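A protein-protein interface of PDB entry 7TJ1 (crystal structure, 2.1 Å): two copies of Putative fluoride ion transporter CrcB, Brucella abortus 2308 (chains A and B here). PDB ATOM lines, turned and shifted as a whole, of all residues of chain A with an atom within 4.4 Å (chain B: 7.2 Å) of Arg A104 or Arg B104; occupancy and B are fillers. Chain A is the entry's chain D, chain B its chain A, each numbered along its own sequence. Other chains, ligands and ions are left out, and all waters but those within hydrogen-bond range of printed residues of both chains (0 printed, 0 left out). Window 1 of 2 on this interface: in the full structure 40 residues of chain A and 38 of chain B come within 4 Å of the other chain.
Of the 12 printed residues of chain A, 9 touch a printed residue of chain B.
Hydrophobic or aromatic side chains of chain A within 4 Å of the printed part of chain B: Leu A78, Ile A80 and Leu A99.
Along chain A the printed residues that touch a printed residue of chain B span positions 78 to 120.
Printed residues of chain B that touch a printed residue of chain A: Leu B78, Ile B80, Gly B98, Leu B99, Asp B100, Leu B101, Arg B104, Ala B105, Leu B106, Thr B118, Asn B120 and Arg B128.
Hydrophobic or aromatic side chains of chain B within 4 Å of the printed part of chain A: Leu B78, Ile B80, Leu B99 and Leu B106.
Along chain B the printed residues that touch a printed residue of chain A span positions 78 to 128.
Among the printed residues, 19 pairs touch across the chains.
Among the printed residues, Asp or Glu carboxylates within 4 Å of a Lys or Arg side-chain nitrogen of the other chain: Asp A100 with Arg B104 and Arg A104 with Asp B100.
Leu A78 touches Leu B99.
Leu A78 touches Leu B101 (CD2 to O, 3.4 Å).
Ile A80 touches Ile B80 (CD1 to CD1, 3.7 Å).
CD1 of Leu B78 touches O of Leu A99, at 3.9 Å.
Ala B105 touches Leu A99.
CD1 of Leu A99 touches O of Thr B118 (3.6 Å).
Leu A99 touches Asn B120 (CD2 to OD1, 3.7 Å).
Arg A104 touches Arg B104.
Leu B99 touches Ala A105 (CD1 to N, 3.7 Å).
Asn A120 touches Leu B99 (OD1 to CD2, 3.6 Å).
NH2 of Arg B104 sits close to ND2 of Asn B120, at 3.4 Å.
ND2 of Asn A120 lies close to NH2 of Arg A104, 3.3 Å away.
The backbone carbonyl oxygen (O) of Leu B106 is in hydrogen-bond range of the backbone NH (N) of Thr B118 (2.8 Å).
The side-chain carboxylate of Asp B100 lies within salt-bridge range of the guanidinium group of Arg B104 (3.7 Å).
The side-chain carboxylate of Asp B100 lies within salt-bridge range of the guanidinium group of Arg B128.
N of Ile A79 sits at hydrogen-bond distance from O of Ala A105, 2.9 Å away.
Printed residues of chain B within 4 Å of Leu A99: Leu B78, Arg B104, Ala B105, Leu B106, Thr B118 and Asn B120.
Printed residues of chain B within 4 Å of Arg A104: Leu B99, Asp B100 and Arg B104.
Printed residues of chain B within 4 Å of Thr A118: Leu B99.
Gly B82 touches none of the printed residues of chain A.
Ile B97 touches none of the printed residues of chain A.
Printed residues of chain A within 4 Å of Gly B98: Leu A78 (3.9 Å).
Of the printed residues of chain A, Leu B99 touches Leu A78, Arg A104, Ala A105, Thr A118, Val A119 and Asn A120.
Printed residues of chain A within 4 Å of Leu B101: Leu A78 (3.4 Å).
Of the printed residues of chain A, Arg B104 touches Leu A99 (2.8 Å), Asp A100 (2.9 Å) and Arg A104 (3.98 Å).
The nearest printed residue of chain A that does not touch Arg B104 is Ile A80 (5.9 Å).
The nearest printed residue of chain B that does not touch Leu A99 is Val B119 (4.001 Å).
NH1 of Arg B104 is in hydrogen-bond range of O of Leu A99, at 2.8 Å.
The guanidinium group (NH1) of Arg A104 lies within hydrogen-bond range of the backbone carbonyl oxygen (O) of Leu B99, at 2.8 Å.
The side-chain amide oxygen (OD1) of Asn A120 is in hydrogen-bond range of the guanidinium group (NH2) of Arg B128, at 2.7 Å.
The side-chain carboxylate (OD1) of Asp A100 lies within salt-bridge range of the guanidinium group (NH1) of Arg B104 (2.9 Å).
The guanidinium group (NH1) of Arg A104 lies within salt-bridge range of the side-chain carboxylate (OD1) of Asp B100.
Leu A78 touches Leu B99, and with the chains exchanged Leu A99 touches Leu B78.
Leu A99 touches Arg B104, and with the chains exchanged Arg A104 touches Leu B99.
Leu A99 touches Thr B118, and with the chains exchanged Thr A118 touches Leu B99.
Asp A100 touches Arg B104, and with the chains exchanged Arg A104 touches Asp B100.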
ATOM      1  N   LEU A  78      15.997 -33.069 -10.275  1.00  0.00           N
ATOM      2  CA  LEU A  78      17.027 -33.215 -11.290  1.00  0.00           C
ATOM      3  C   LEU A  78      18.333 -33.644 -10.636  1.00  0.00           C
ATOM      4  O   LEU A  78      18.646 -33.220  -9.520  1.00  0.00           O
ATOM      5  CB  LEU A  78      17.231 -31.895 -12.037  1.00  0.00           C
ATOM      6  CG  LEU A  78      18.344 -31.830 -13.082  1.00  0.00           C
ATOM      7  CD1 LEU A  78      17.931 -32.573 -14.344  1.00  0.00           C
ATOM      8  CD2 LEU A  78      18.696 -30.381 -13.388  1.00  0.00           C
ATOM      9  N   ILE A  79      19.094 -34.488 -11.329  1.00  0.00           N
ATOM     10  CA  ILE A  79      20.416 -34.894 -10.868  1.00  0.00           C
ATOM     11  C   ILE A  79      21.392 -34.770 -12.029  1.00  0.00           C
ATOM     12  O   ILE A  79      21.046 -35.055 -13.181  1.00  0.00           O
ATOM     13  CB  ILE A  79      20.417 -36.325 -10.278  1.00  0.00           C
ATOM     14  CG1 ILE A  79      21.796 -36.660  -9.704  1.00  0.00           C
ATOM     15  CG2 ILE A  79      20.007 -37.351 -11.321  1.00  0.00           C
ATOM     16  CD1 ILE A  79      21.827 -37.923  -8.867  1.00  0.00           C
ATOM     17  N   ILE A  80      22.609 -34.323 -11.723  1.00  0.00           N
ATOM     18  CA  ILE A  80      23.633 -34.035 -12.721  1.00  0.00           C
ATOM     19  C   ILE A  80      24.865 -34.866 -12.384  1.00  0.00           C
ATOM     20  O   ILE A  80      25.399 -34.774 -11.272  1.00  0.00           O
ATOM     21  CB  ILE A  80      23.966 -32.536 -12.771  1.00  0.00           C
ATOM     22  CG1 ILE A  80      22.704 -31.735 -13.112  1.00  0.00           C
ATOM     23  CG2 ILE A  80      25.071 -32.266 -13.780  1.00  0.00           C
ATOM     24  CD1 ILE A  80      22.929 -30.249 -13.233  1.00  0.00           C
ATOM     25  N   LEU A  99      27.581 -26.965 -22.538  1.00  0.00           N
ATOM     26  CA  LEU A  99      26.346 -26.394 -22.016  1.00  0.00           C
ATOM     27  C   LEU A  99      25.365 -27.481 -21.600  1.00  0.00           C
ATOM     28  O   LEU A  99      24.595 -27.290 -20.652  1.00  0.00           O
ATOM     29  CB  LEU A  99      25.709 -25.482 -23.065  1.00  0.00           C
ATOM     30  CG  LEU A  99      24.344 -24.864 -22.738  1.00  0.00           C
ATOM     31  CD1 LEU A  99      24.478 -23.777 -21.678  1.00  0.00           C
ATOM     32  CD2 LEU A  99      23.680 -24.317 -24.000  1.00  0.00           C
ATOM     33  N   ASP A 100      25.381 -28.618 -22.290  1.00  0.00           N
ATOM     34  CA  ASP A 100      24.449 -29.707 -22.037  1.00  0.00           C
ATOM     35  C   ASP A 100      25.069 -30.842 -21.238  1.00  0.00           C
ATOM     36  O   ASP A 100      24.406 -31.858 -21.010  1.00  0.00           O
ATOM     37  CB  ASP A 100      23.890 -30.238 -23.364  1.00  0.00           C
ATOM     38  CG  ASP A 100      22.967 -29.241 -24.046  1.00  0.00           C
ATOM     39  OD1 ASP A 100      22.327 -28.445 -23.327  1.00  0.00           O
ATOM     40  OD2 ASP A 100      22.878 -29.250 -25.295  1.00  0.00           O
ATOM     41  N   PRO A 102      27.344 -31.722 -17.479  1.00  0.00           N
ATOM     42  CA  PRO A 102      27.274 -33.187 -17.378  1.00  0.00           C
ATOM     43  C   PRO A 102      25.884 -33.775 -17.640  1.00  0.00           C
ATOM     44  O   PRO A 102      24.914 -33.028 -17.808  1.00  0.00           O
ATOM     45  CB  PRO A 102      27.705 -33.460 -15.928  1.00  0.00           C
ATOM     46  CG  PRO A 102      28.389 -32.201 -15.473  1.00  0.00           C
ATOM     47  CD  PRO A 102      27.666 -31.107 -16.183  1.00  0.00           C
ATOM     48  N   ILE A 103      25.813 -35.109 -17.680  1.00  0.00           N
ATOM     49  CA  ILE A 103      24.558 -35.794 -17.966  1.00  0.00           C
ATOM     50  C   ILE A 103      23.502 -35.389 -16.948  1.00  0.00           C
ATOM     51  O   ILE A 103      23.780 -35.247 -15.752  1.00  0.00           O
ATOM     52  CB  ILE A 103      24.771 -37.317 -17.966  1.00  0.00           C
ATOM     53  CG1 ILE A 103      25.958 -37.690 -18.857  1.00  0.00           C
ATOM     54  CG2 ILE A 103      23.516 -38.036 -18.441  1.00  0.00           C
ATOM     55  CD1 ILE A 103      26.338 -39.154 -18.781  1.00  0.00           C
ATOM     56  N   ARG A 104      22.278 -35.191 -17.428  1.00  0.00           N
ATOM     57  CA  ARG A 104      21.163 -34.779 -16.591  1.00  0.00           C
ATOM     58  C   ARG A 104      20.059 -35.827 -16.646  1.00  0.00           C
ATOM     59  O   ARG A 104      19.788 -36.405 -17.703  1.00  0.00           O
ATOM     60  CB  ARG A 104      20.621 -33.413 -17.031  1.00  0.00           C
ATOM     61  CG  ARG A 104      21.485 -32.239 -16.582  1.00  0.00           C
ATOM     62  CD  ARG A 104      21.126 -30.950 -17.318  1.00  0.00           C
ATOM     63  NE  ARG A 104      21.595 -30.971 -18.699  1.00  0.00           N
ATOM     64  CZ  ARG A 104      20.809 -31.028 -19.764  1.00  0.00           C
ATOM     65  NH1 ARG A 104      19.491 -31.033 -19.653  1.00  0.00           N
ATOM     66  NH2 ARG A 104      21.359 -31.073 -20.974  1.00  0.00           N
ATOM     67  N   ALA A 105      19.435 -36.073 -15.498  1.00  0.00           N
ATOM     68  CA  ALA A 105      18.294 -36.971 -15.405  1.00  0.00           C
ATOM     69  C   ALA A 105      17.245 -36.335 -14.509  1.00  0.00           C
ATOM     70  O   ALA A 105      17.575 -35.754 -13.471  1.00  0.00           O
ATOM     71  CB  ALA A 105      18.696 -38.346 -14.859  1.00  0.00           C
ATOM     72  N   THR A 118      13.335 -39.159 -16.978  1.00  0.00           N
ATOM     73  CA  THR A 118      13.578 -38.561 -18.284  1.00  0.00           C
ATOM     74  C   THR A 118      15.054 -38.207 -18.416  1.00  0.00           C
ATOM     75  O   THR A 118      15.635 -37.608 -17.505  1.00  0.00           O
ATOM     76  CB  THR A 118      12.713 -37.311 -18.482  1.00  0.00           C
ATOM     77  OG1 THR A 118      11.328 -37.669 -18.413  1.00  0.00           O
ATOM     78  CG2 THR A 118      12.995 -36.662 -19.832  1.00  0.00           C
ATOM     79  N   VAL A 119      15.657 -38.581 -19.549  1.00  0.00           N
ATOM     80  CA  VAL A 119      17.054 -38.281 -19.846  1.00  0.00           C
ATOM     81  C   VAL A 119      17.163 -37.823 -21.296  1.00  0.00           C
ATOM     82  O   VAL A 119      16.229 -37.961 -22.089  1.00  0.00           O
ATOM     83  CB  VAL A 119      17.988 -39.487 -19.604  1.00  0.00           C
ATOM     84  CG1 VAL A 119      17.947 -39.931 -18.143  1.00  0.00           C
ATOM     85  CG2 VAL A 119      17.620 -40.636 -20.530  1.00  0.00           C
ATOM     86  N   ASN A 120      18.328 -37.275 -21.635  1.00  0.00           N
ATOM     87  CA  ASN A 120      18.637 -36.902 -23.010  1.00  0.00           C
ATOM     88  C   ASN A 120      19.171 -38.099 -23.786  1.00  0.00           C
ATOM     89  O   ASN A 120      19.955 -38.897 -23.263  1.00  0.00           O
ATOM     90  CB  ASN A 120      19.680 -35.783 -23.046  1.00  0.00           C
ATOM     91  CG  ASN A 120      19.139 -34.456 -22.562  1.00  0.00           C
ATOM     92  OD1 ASN A 120      18.156 -33.943 -23.094  1.00  0.00           O
ATOM     93  ND2 ASN A 120      19.783 -33.889 -21.545  1.00  0.00           N
ATOM     94  N   VAL B  45      27.532 -13.138 -14.875  1.00  0.00           N
ATOM     95  CA  VAL B  45      26.256 -13.843 -14.963  1.00  0.00           C
ATOM     96  C   VAL B  45      25.635 -13.975 -13.579  1.00  0.00           C
ATOM     97  O   VAL B  45      24.458 -13.654 -13.371  1.00  0.00           O
ATOM     98  CB  VAL B  45      26.440 -15.222 -15.625  1.00  0.00           C
ATOM     99  CG1 VAL B  45      25.161 -16.032 -15.497  1.00  0.00           C
ATOM    100  CG2 VAL B  45      26.831 -15.080 -17.087  1.00  0.00           C
ATOM    101  N   LEU B  78      30.527 -23.736 -16.618  1.00  0.00           N
ATOM    102  CA  LEU B  78      29.075 -23.750 -16.708  1.00  0.00           C
ATOM    103  C   LEU B  78      28.492 -23.188 -15.419  1.00  0.00           C
ATOM    104  O   LEU B  78      28.957 -23.520 -14.324  1.00  0.00           O
ATOM    105  CB  LEU B  78      28.558 -25.173 -16.930  1.00  0.00           C
ATOM    106  CG  LEU B  78      27.042 -25.372 -16.937  1.00  0.00           C
ATOM    107  CD1 LEU B  78      26.458 -24.872 -18.252  1.00  0.00           C
ATOM    108  CD2 LEU B  78      26.694 -26.835 -16.699  1.00  0.00           C
ATOM    109  N   ILE B  79      27.482 -22.334 -15.546  1.00  0.00           N
ATOM    110  CA  ILE B  79      26.778 -21.794 -14.390  1.00  0.00           C
ATOM    111  C   ILE B  79      25.294 -22.086 -14.553  1.00  0.00           C
ATOM    112  O   ILE B  79      24.755 -22.032 -15.665  1.00  0.00           O
ATOM    113  CB  ILE B  79      27.041 -20.283 -14.196  1.00  0.00           C
ATOM    114  CG1 ILE B  79      26.394 -19.793 -12.897  1.00  0.00           C
ATOM    115  CG2 ILE B  79      26.547 -19.483 -15.392  1.00  0.00           C
ATOM    116  CD1 ILE B  79      27.002 -18.526 -12.332  1.00  0.00           C
ATOM    117  N   ILE B  80      24.644 -22.430 -13.444  1.00  0.00           N
ATOM    118  CA  ILE B  80      23.244 -22.832 -13.431  1.00  0.00           C
ATOM    119  C   ILE B  80      22.499 -21.887 -12.500  1.00  0.00           C
ATOM    120  O   ILE B  80      22.842 -21.773 -11.317  1.00  0.00           O
ATOM    121  CB  ILE B  80      23.081 -24.295 -12.992  1.00  0.00           C
ATOM    122  CG1 ILE B  80      23.859 -25.212 -13.943  1.00  0.00           C
ATOM    123  CG2 ILE B  80      21.606 -24.680 -12.930  1.00  0.00           C
ATOM    124  CD1 ILE B  80      23.657 -26.685 -13.687  1.00  0.00           C
ATOM    125  N   PHE B  81      21.484 -21.212 -13.035  1.00  0.00           N
ATOM    126  CA  PHE B  81      20.779 -20.167 -12.309  1.00  0.00           C
ATOM    127  C   PHE B  81      19.341 -20.106 -12.802  1.00  0.00           C
ATOM    128  O   PHE B  81      19.017 -20.614 -13.879  1.00  0.00           O
ATOM    129  CB  PHE B  81      21.463 -18.806 -12.492  1.00  0.00           C
ATOM    130  CG  PHE B  81      21.465 -18.321 -13.915  1.00  0.00           C
ATOM    131  CD1 PHE B  81      22.453 -18.731 -14.800  1.00  0.00           C
ATOM    132  CD2 PHE B  81      20.475 -17.464 -14.371  1.00  0.00           C
ATOM    133  CE1 PHE B  81      22.455 -18.293 -16.112  1.00  0.00           C
ATOM    134  CE2 PHE B  81      20.471 -17.019 -15.680  1.00  0.00           C
ATOM    135  CZ  PHE B  81      21.463 -17.435 -16.553  1.00  0.00           C
ATOM    136  N   GLY B  82      18.482 -19.470 -12.015  1.00  0.00           N
ATOM    137  CA  GLY B  82      17.106 -19.300 -12.446  1.00  0.00           C
ATOM    138  C   GLY B  82      16.207 -18.846 -11.319  1.00  0.00           C
ATOM    139  O   GLY B  82      16.567 -18.877 -10.139  1.00  0.00           O
ATOM    140  N   ILE B  97      10.490 -30.260 -19.053  1.00  0.00           N
ATOM    141  CA  ILE B  97      11.388 -29.119 -19.190  1.00  0.00           C
ATOM    142  C   ILE B  97      12.244 -28.941 -17.939  1.00  0.00           C
ATOM    143  O   ILE B  97      13.271 -28.254 -17.983  1.00  0.00           O
ATOM    144  CB  ILE B  97      10.608 -27.831 -19.521  1.00  0.00           C
ATOM    145  CG1 ILE B  97      11.562 -26.752 -20.050  1.00  0.00           C
ATOM    146  CG2 ILE B  97       9.848 -27.329 -18.302  1.00  0.00           C
ATOM    147  CD1 ILE B  97      10.868 -25.489 -20.518  1.00  0.00           C
ATOM    148  N   GLY B  98      11.857 -29.565 -16.822  1.00  0.00           N
ATOM    149  CA  GLY B  98      12.711 -29.593 -15.647  1.00  0.00           C
ATOM    150  C   GLY B  98      14.038 -30.286 -15.879  1.00  0.00           C
ATOM    151  O   GLY B  98      14.962 -30.126 -15.074  1.00  0.00           O
ATOM    152  N   LEU B  99      14.151 -31.064 -16.957  1.00  0.00           N
ATOM    153  CA  LEU B  99      15.441 -31.634 -17.330  1.00  0.00           C
ATOM    154  C   LEU B  99      16.406 -30.559 -17.807  1.00  0.00           C
ATOM    155  O   LEU B  99      17.619 -30.677 -17.595  1.00  0.00           O
ATOM    156  CB  LEU B  99      15.253 -32.691 -18.420  1.00  0.00           C
ATOM    157  CG  LEU B  99      16.495 -33.444 -18.901  1.00  0.00           C
ATOM    158  CD1 LEU B  99      17.040 -34.351 -17.805  1.00  0.00           C
ATOM    159  CD2 LEU B  99      16.179 -34.242 -20.160  1.00  0.00           C
ATOM    160  N   ASP B 100      15.891 -29.509 -18.441  1.00  0.00           N
ATOM    161  CA  ASP B 100      16.702 -28.448 -19.023  1.00  0.00           C
ATOM    162  C   ASP B 100      16.700 -27.173 -18.192  1.00  0.00           C
ATOM    163  O   ASP B 100      17.294 -26.175 -18.611  1.00  0.00           O
ATOM    164  CB  ASP B 100      16.220 -28.139 -20.447  1.00  0.00           C
ATOM    165  CG  ASP B 100      16.441 -29.299 -21.403  1.00  0.00           C
ATOM    166  OD1 ASP B 100      17.407 -30.062 -21.190  1.00  0.00           O
ATOM    167  OD2 ASP B 100      15.653 -29.451 -22.364  1.00  0.00           O
ATOM    168  N   LEU B 101      16.032 -27.177 -17.040  1.00  0.00           N
ATOM    169  CA  LEU B 101      16.036 -26.098 -16.069  1.00  0.00           C
ATOM    170  C   LEU B 101      16.827 -26.511 -14.830  1.00  0.00           C
ATOM    171  O   LEU B 101      16.931 -27.706 -14.533  1.00  0.00           O
ATOM    172  CB  LEU B 101      14.606 -25.723 -15.661  1.00  0.00           C
ATOM    173  CG  LEU B 101      13.717 -25.135 -16.758  1.00  0.00           C
ATOM    174  CD1 LEU B 101      12.304 -24.922 -16.238  1.00  0.00           C
ATOM    175  CD2 LEU B 101      14.305 -23.832 -17.282  1.00  0.00           C
ATOM    176  N   PRO B 102      17.405 -25.556 -14.077  1.00  0.00           N
ATOM    177  CA  PRO B 102      17.393 -24.101 -14.271  1.00  0.00           C
ATOM    178  C   PRO B 102      18.241 -23.660 -15.460  1.00  0.00           C
ATOM    179  O   PRO B 102      18.892 -24.502 -16.085  1.00  0.00           O
ATOM    180  CB  PRO B 102      17.981 -23.560 -12.958  1.00  0.00           C
ATOM    181  CG  PRO B 102      17.949 -24.712 -11.999  1.00  0.00           C
ATOM    182  CD  PRO B 102      18.119 -25.926 -12.846  1.00  0.00           C
ATOM    183  N   ILE B 103      18.225 -22.356 -15.755  1.00  0.00           N
ATOM    184  CA  ILE B 103      18.924 -21.838 -16.924  1.00  0.00           C
ATOM    185  C   ILE B 103      20.409 -22.153 -16.829  1.00  0.00           C
ATOM    186  O   ILE B 103      21.028 -22.028 -15.764  1.00  0.00           O
ATOM    187  CB  ILE B 103      18.694 -20.323 -17.061  1.00  0.00           C
ATOM    188  CG1 ILE B 103      17.201 -19.999 -16.982  1.00  0.00           C
ATOM    189  CG2 ILE B 103      19.291 -19.806 -18.363  1.00  0.00           C
ATOM    190  CD1 ILE B 103      16.908 -18.523 -16.833  1.00  0.00           C
ATOM    191  N   ARG B 104      20.984 -22.573 -17.950  1.00  0.00           N
ATOM    192  CA  ARG B 104      22.398 -22.894 -18.049  1.00  0.00           C
ATOM    193  C   ARG B 104      23.088 -21.908 -18.983  1.00  0.00           C
ATOM    194  O   ARG B 104      22.519 -21.501 -20.001  1.00  0.00           O
ATOM    195  CB  ARG B 104      22.598 -24.326 -18.549  1.00  0.00           C
ATOM    196  CG  ARG B 104      22.506 -25.372 -17.447  1.00  0.00           C
ATOM    197  CD  ARG B 104      22.270 -26.766 -18.005  1.00  0.00           C
ATOM    198  NE  ARG B 104      20.965 -26.875 -18.644  1.00  0.00           N
ATOM    199  CZ  ARG B 104      20.777 -27.030 -19.948  1.00  0.00           C
ATOM    200  NH1 ARG B 104      21.796 -27.117 -20.787  1.00  0.00           N
ATOM    201  NH2 ARG B 104      19.537 -27.108 -20.419  1.00  0.00           N
ATOM    202  N   ALA B 105      24.311 -21.525 -18.624  1.00  0.00           N
ATOM    203  CA  ALA B 105      25.124 -20.623 -19.428  1.00  0.00           C
ATOM    204  C   ALA B 105      26.558 -21.127 -19.409  1.00  0.00           C
ATOM    205  O   ALA B 105      27.088 -21.446 -18.341  1.00  0.00           O
ATOM    206  CB  ALA B 105      25.061 -19.184 -18.901  1.00  0.00           C
ATOM    207  N   LEU B 106      27.178 -21.201 -20.584  1.00  0.00           N
ATOM    208  CA  LEU B 106      28.526 -21.733 -20.726  1.00  0.00           C
ATOM    209  C   LEU B 106      29.455 -20.625 -21.196  1.00  0.00           C
ATOM    210  O   LEU B 106      29.271 -20.083 -22.290  1.00  0.00           O
ATOM    211  CB  LEU B 106      28.557 -22.901 -21.713  1.00  0.00           C
ATOM    212  CG  LEU B 106      29.936 -23.530 -21.907  1.00  0.00           C
ATOM    213  CD1 LEU B 106      30.317 -24.365 -20.681  1.00  0.00           C
ATOM    214  CD2 LEU B 106      29.977 -24.360 -23.184  1.00  0.00           C
ATOM    215  N   LEU B 117      30.160 -16.799 -24.785  1.00  0.00           N
ATOM    216  CA  LEU B 117      29.110 -17.090 -23.814  1.00  0.00           C
ATOM    217  C   LEU B 117      27.938 -17.707 -24.560  1.00  0.00           C
ATOM    218  O   LEU B 117      27.382 -17.082 -25.466  1.00  0.00           O
ATOM    219  CB  LEU B 117      28.676 -15.824 -23.069  1.00  0.00           C
ATOM    220  CG  LEU B 117      27.587 -15.986 -22.006  1.00  0.00           C
ATOM    221  CD1 LEU B 117      28.015 -16.989 -20.945  1.00  0.00           C
ATOM    222  CD2 LEU B 117      27.248 -14.645 -21.367  1.00  0.00           C
ATOM    223  N   THR B 118      27.564 -18.926 -24.177  1.00  0.00           N
ATOM    224  CA  THR B 118      26.576 -19.718 -24.898  1.00  0.00           C
ATOM    225  C   THR B 118      25.415 -20.066 -23.976  1.00  0.00           C
ATOM    226  O   THR B 118      25.630 -20.525 -22.850  1.00  0.00           O
ATOM    227  CB  THR B 118      27.214 -20.995 -25.449  1.00  0.00           C
ATOM    228  OG1 THR B 118      28.258 -20.643 -26.364  1.00  0.00           O
ATOM    229  CG2 THR B 118      26.180 -21.859 -26.162  1.00  0.00           C
ATOM    230  N   VAL B 119      24.187 -19.854 -24.461  1.00  0.00           N
ATOM    231  CA  VAL B 119      22.973 -20.158 -23.712  1.00  0.00           C
ATOM    232  C   VAL B 119      21.945 -20.772 -24.655  1.00  0.00           C
ATOM    233  O   VAL B 119      22.061 -20.686 -25.880  1.00  0.00           O
ATOM    234  CB  VAL B 119      22.370 -18.904 -23.035  1.00  0.00           C
ATOM    235  CG1 VAL B 119      23.344 -18.304 -22.035  1.00  0.00           C
ATOM    236  CG2 VAL B 119      21.970 -17.873 -24.089  1.00  0.00           C
ATOM    237  N   ASN B 120      20.924 -21.391 -24.066  1.00  0.00           N
ATOM    238  CA  ASN B 120      19.791 -21.885 -24.840  1.00  0.00           C
ATOM    239  C   ASN B 120      18.845 -20.745 -25.186  1.00  0.00           C
ATOM    240  O   ASN B 120      18.581 -19.863 -24.362  1.00  0.00           O
ATOM    241  CB  ASN B 120      19.014 -22.954 -24.071  1.00  0.00           C
ATOM    242  CG  ASN B 120      19.799 -24.232 -23.883  1.00  0.00           C
ATOM    243  OD1 ASN B 120      20.103 -24.933 -24.847  1.00  0.00           O
ATOM    244  ND2 ASN B 120      20.112 -24.556 -22.635  1.00  0.00           N
ATOM    245  N   TRP B 124      13.315 -21.925 -28.276  1.00  0.00           N
ATOM    246  CA  TRP B 124      13.682 -23.262 -28.732  1.00  0.00           C
ATOM    247  C   TRP B 124      13.406 -24.305 -27.655  1.00  0.00           C
ATOM    248  O   TRP B 124      12.938 -25.410 -27.957  1.00  0.00           O
ATOM    249  CB  TRP B 124      15.157 -23.274 -29.141  1.00  0.00           C
ATOM    250  CG  TRP B 124      15.667 -24.590 -29.647  1.00  0.00           C
ATOM    251  CD1 TRP B 124      15.703 -25.013 -30.945  1.00  0.00           C
ATOM    252  CD2 TRP B 124      16.244 -25.645 -28.866  1.00  0.00           C
ATOM    253  NE1 TRP B 124      16.254 -26.271 -31.018  1.00  0.00           N
ATOM    254  CE2 TRP B 124      16.596 -26.681 -29.756  1.00  0.00           C
ATOM    255  CE3 TRP B 124      16.491 -25.817 -27.501  1.00  0.00           C
ATOM    256  CZ2 TRP B 124      17.180 -27.870 -29.326  1.00  0.00           C
ATOM    257  CZ3 TRP B 124      17.073 -27.002 -27.074  1.00  0.00           C
ATOM    258  CH2 TRP B 124      17.409 -28.011 -27.984  1.00  0.00           C
ATOM    259  N   LEU B 125      13.686 -23.969 -26.392  1.00  0.00           N
ATOM    260  CA  LEU B 125      13.386 -24.887 -25.296  1.00  0.00           C
ATOM    261  C   LEU B 125      11.888 -25.135 -25.174  1.00  0.00           C
ATOM    262  O   LEU B 125      11.458 -26.266 -24.915  1.00  0.00           O
ATOM    263  CB  LEU B 125      13.938 -24.343 -23.979  1.00  0.00           C
ATOM    264  CG  LEU B 125      15.384 -24.688 -23.638  1.00  0.00           C
ATOM    265  CD1 LEU B 125      15.755 -24.119 -22.277  1.00  0.00           C
ATOM    266  CD2 LEU B 125      15.586 -26.195 -23.672  1.00  0.00           C
ATOM    267  N   ARG B 128      10.985 -27.580 -27.708  1.00  0.00           N
ATOM    268  CA  ARG B 128      11.489 -28.929 -27.457  1.00  0.00           C
ATOM    269  C   ARG B 128      10.533 -29.725 -26.581  1.00  0.00           C
ATOM    270  O   ARG B 128      10.328 -30.923 -26.808  1.00  0.00           O
ATOM    271  CB  ARG B 128      12.873 -28.892 -26.806  1.00  0.00           C
ATOM    272  CG  ARG B 128      13.458 -30.293 -26.669  1.00  0.00           C
ATOM    273  CD  ARG B 128      14.710 -30.376 -25.814  1.00  0.00           C
ATOM    274  NE  ARG B 128      15.289 -31.711 -25.923  1.00  0.00           N
ATOM    275  CZ  ARG B 128      16.118 -32.256 -25.043  1.00  0.00           C
ATOM    276  NH1 ARG B 128      16.485 -31.616 -23.946  1.00  0.00           N
ATOM    277  NH2 ARG B 128      16.585 -33.482 -25.268  1.00  0.00           N
ATOM    278  N   THR B 146      17.158 -14.237 -19.707  1.00  0.00           N
ATOM    279  CA  THR B 146      18.354 -14.749 -20.368  1.00  0.00           C
ATOM    280  C   THR B 146      19.051 -13.656 -21.167  1.00  0.00           C
ATOM    281  O   THR B 146      20.280 -13.527 -21.115  1.00  0.00           O
ATOM    282  CB  THR B 146      17.995 -15.925 -21.276  1.00  0.00           C
ATOM    283  OG1 THR B 146      17.425 -16.979 -20.491  1.00  0.00           O
ATOM    284  CG2 THR B 146      19.237 -16.445 -21.991  1.00  0.00           C
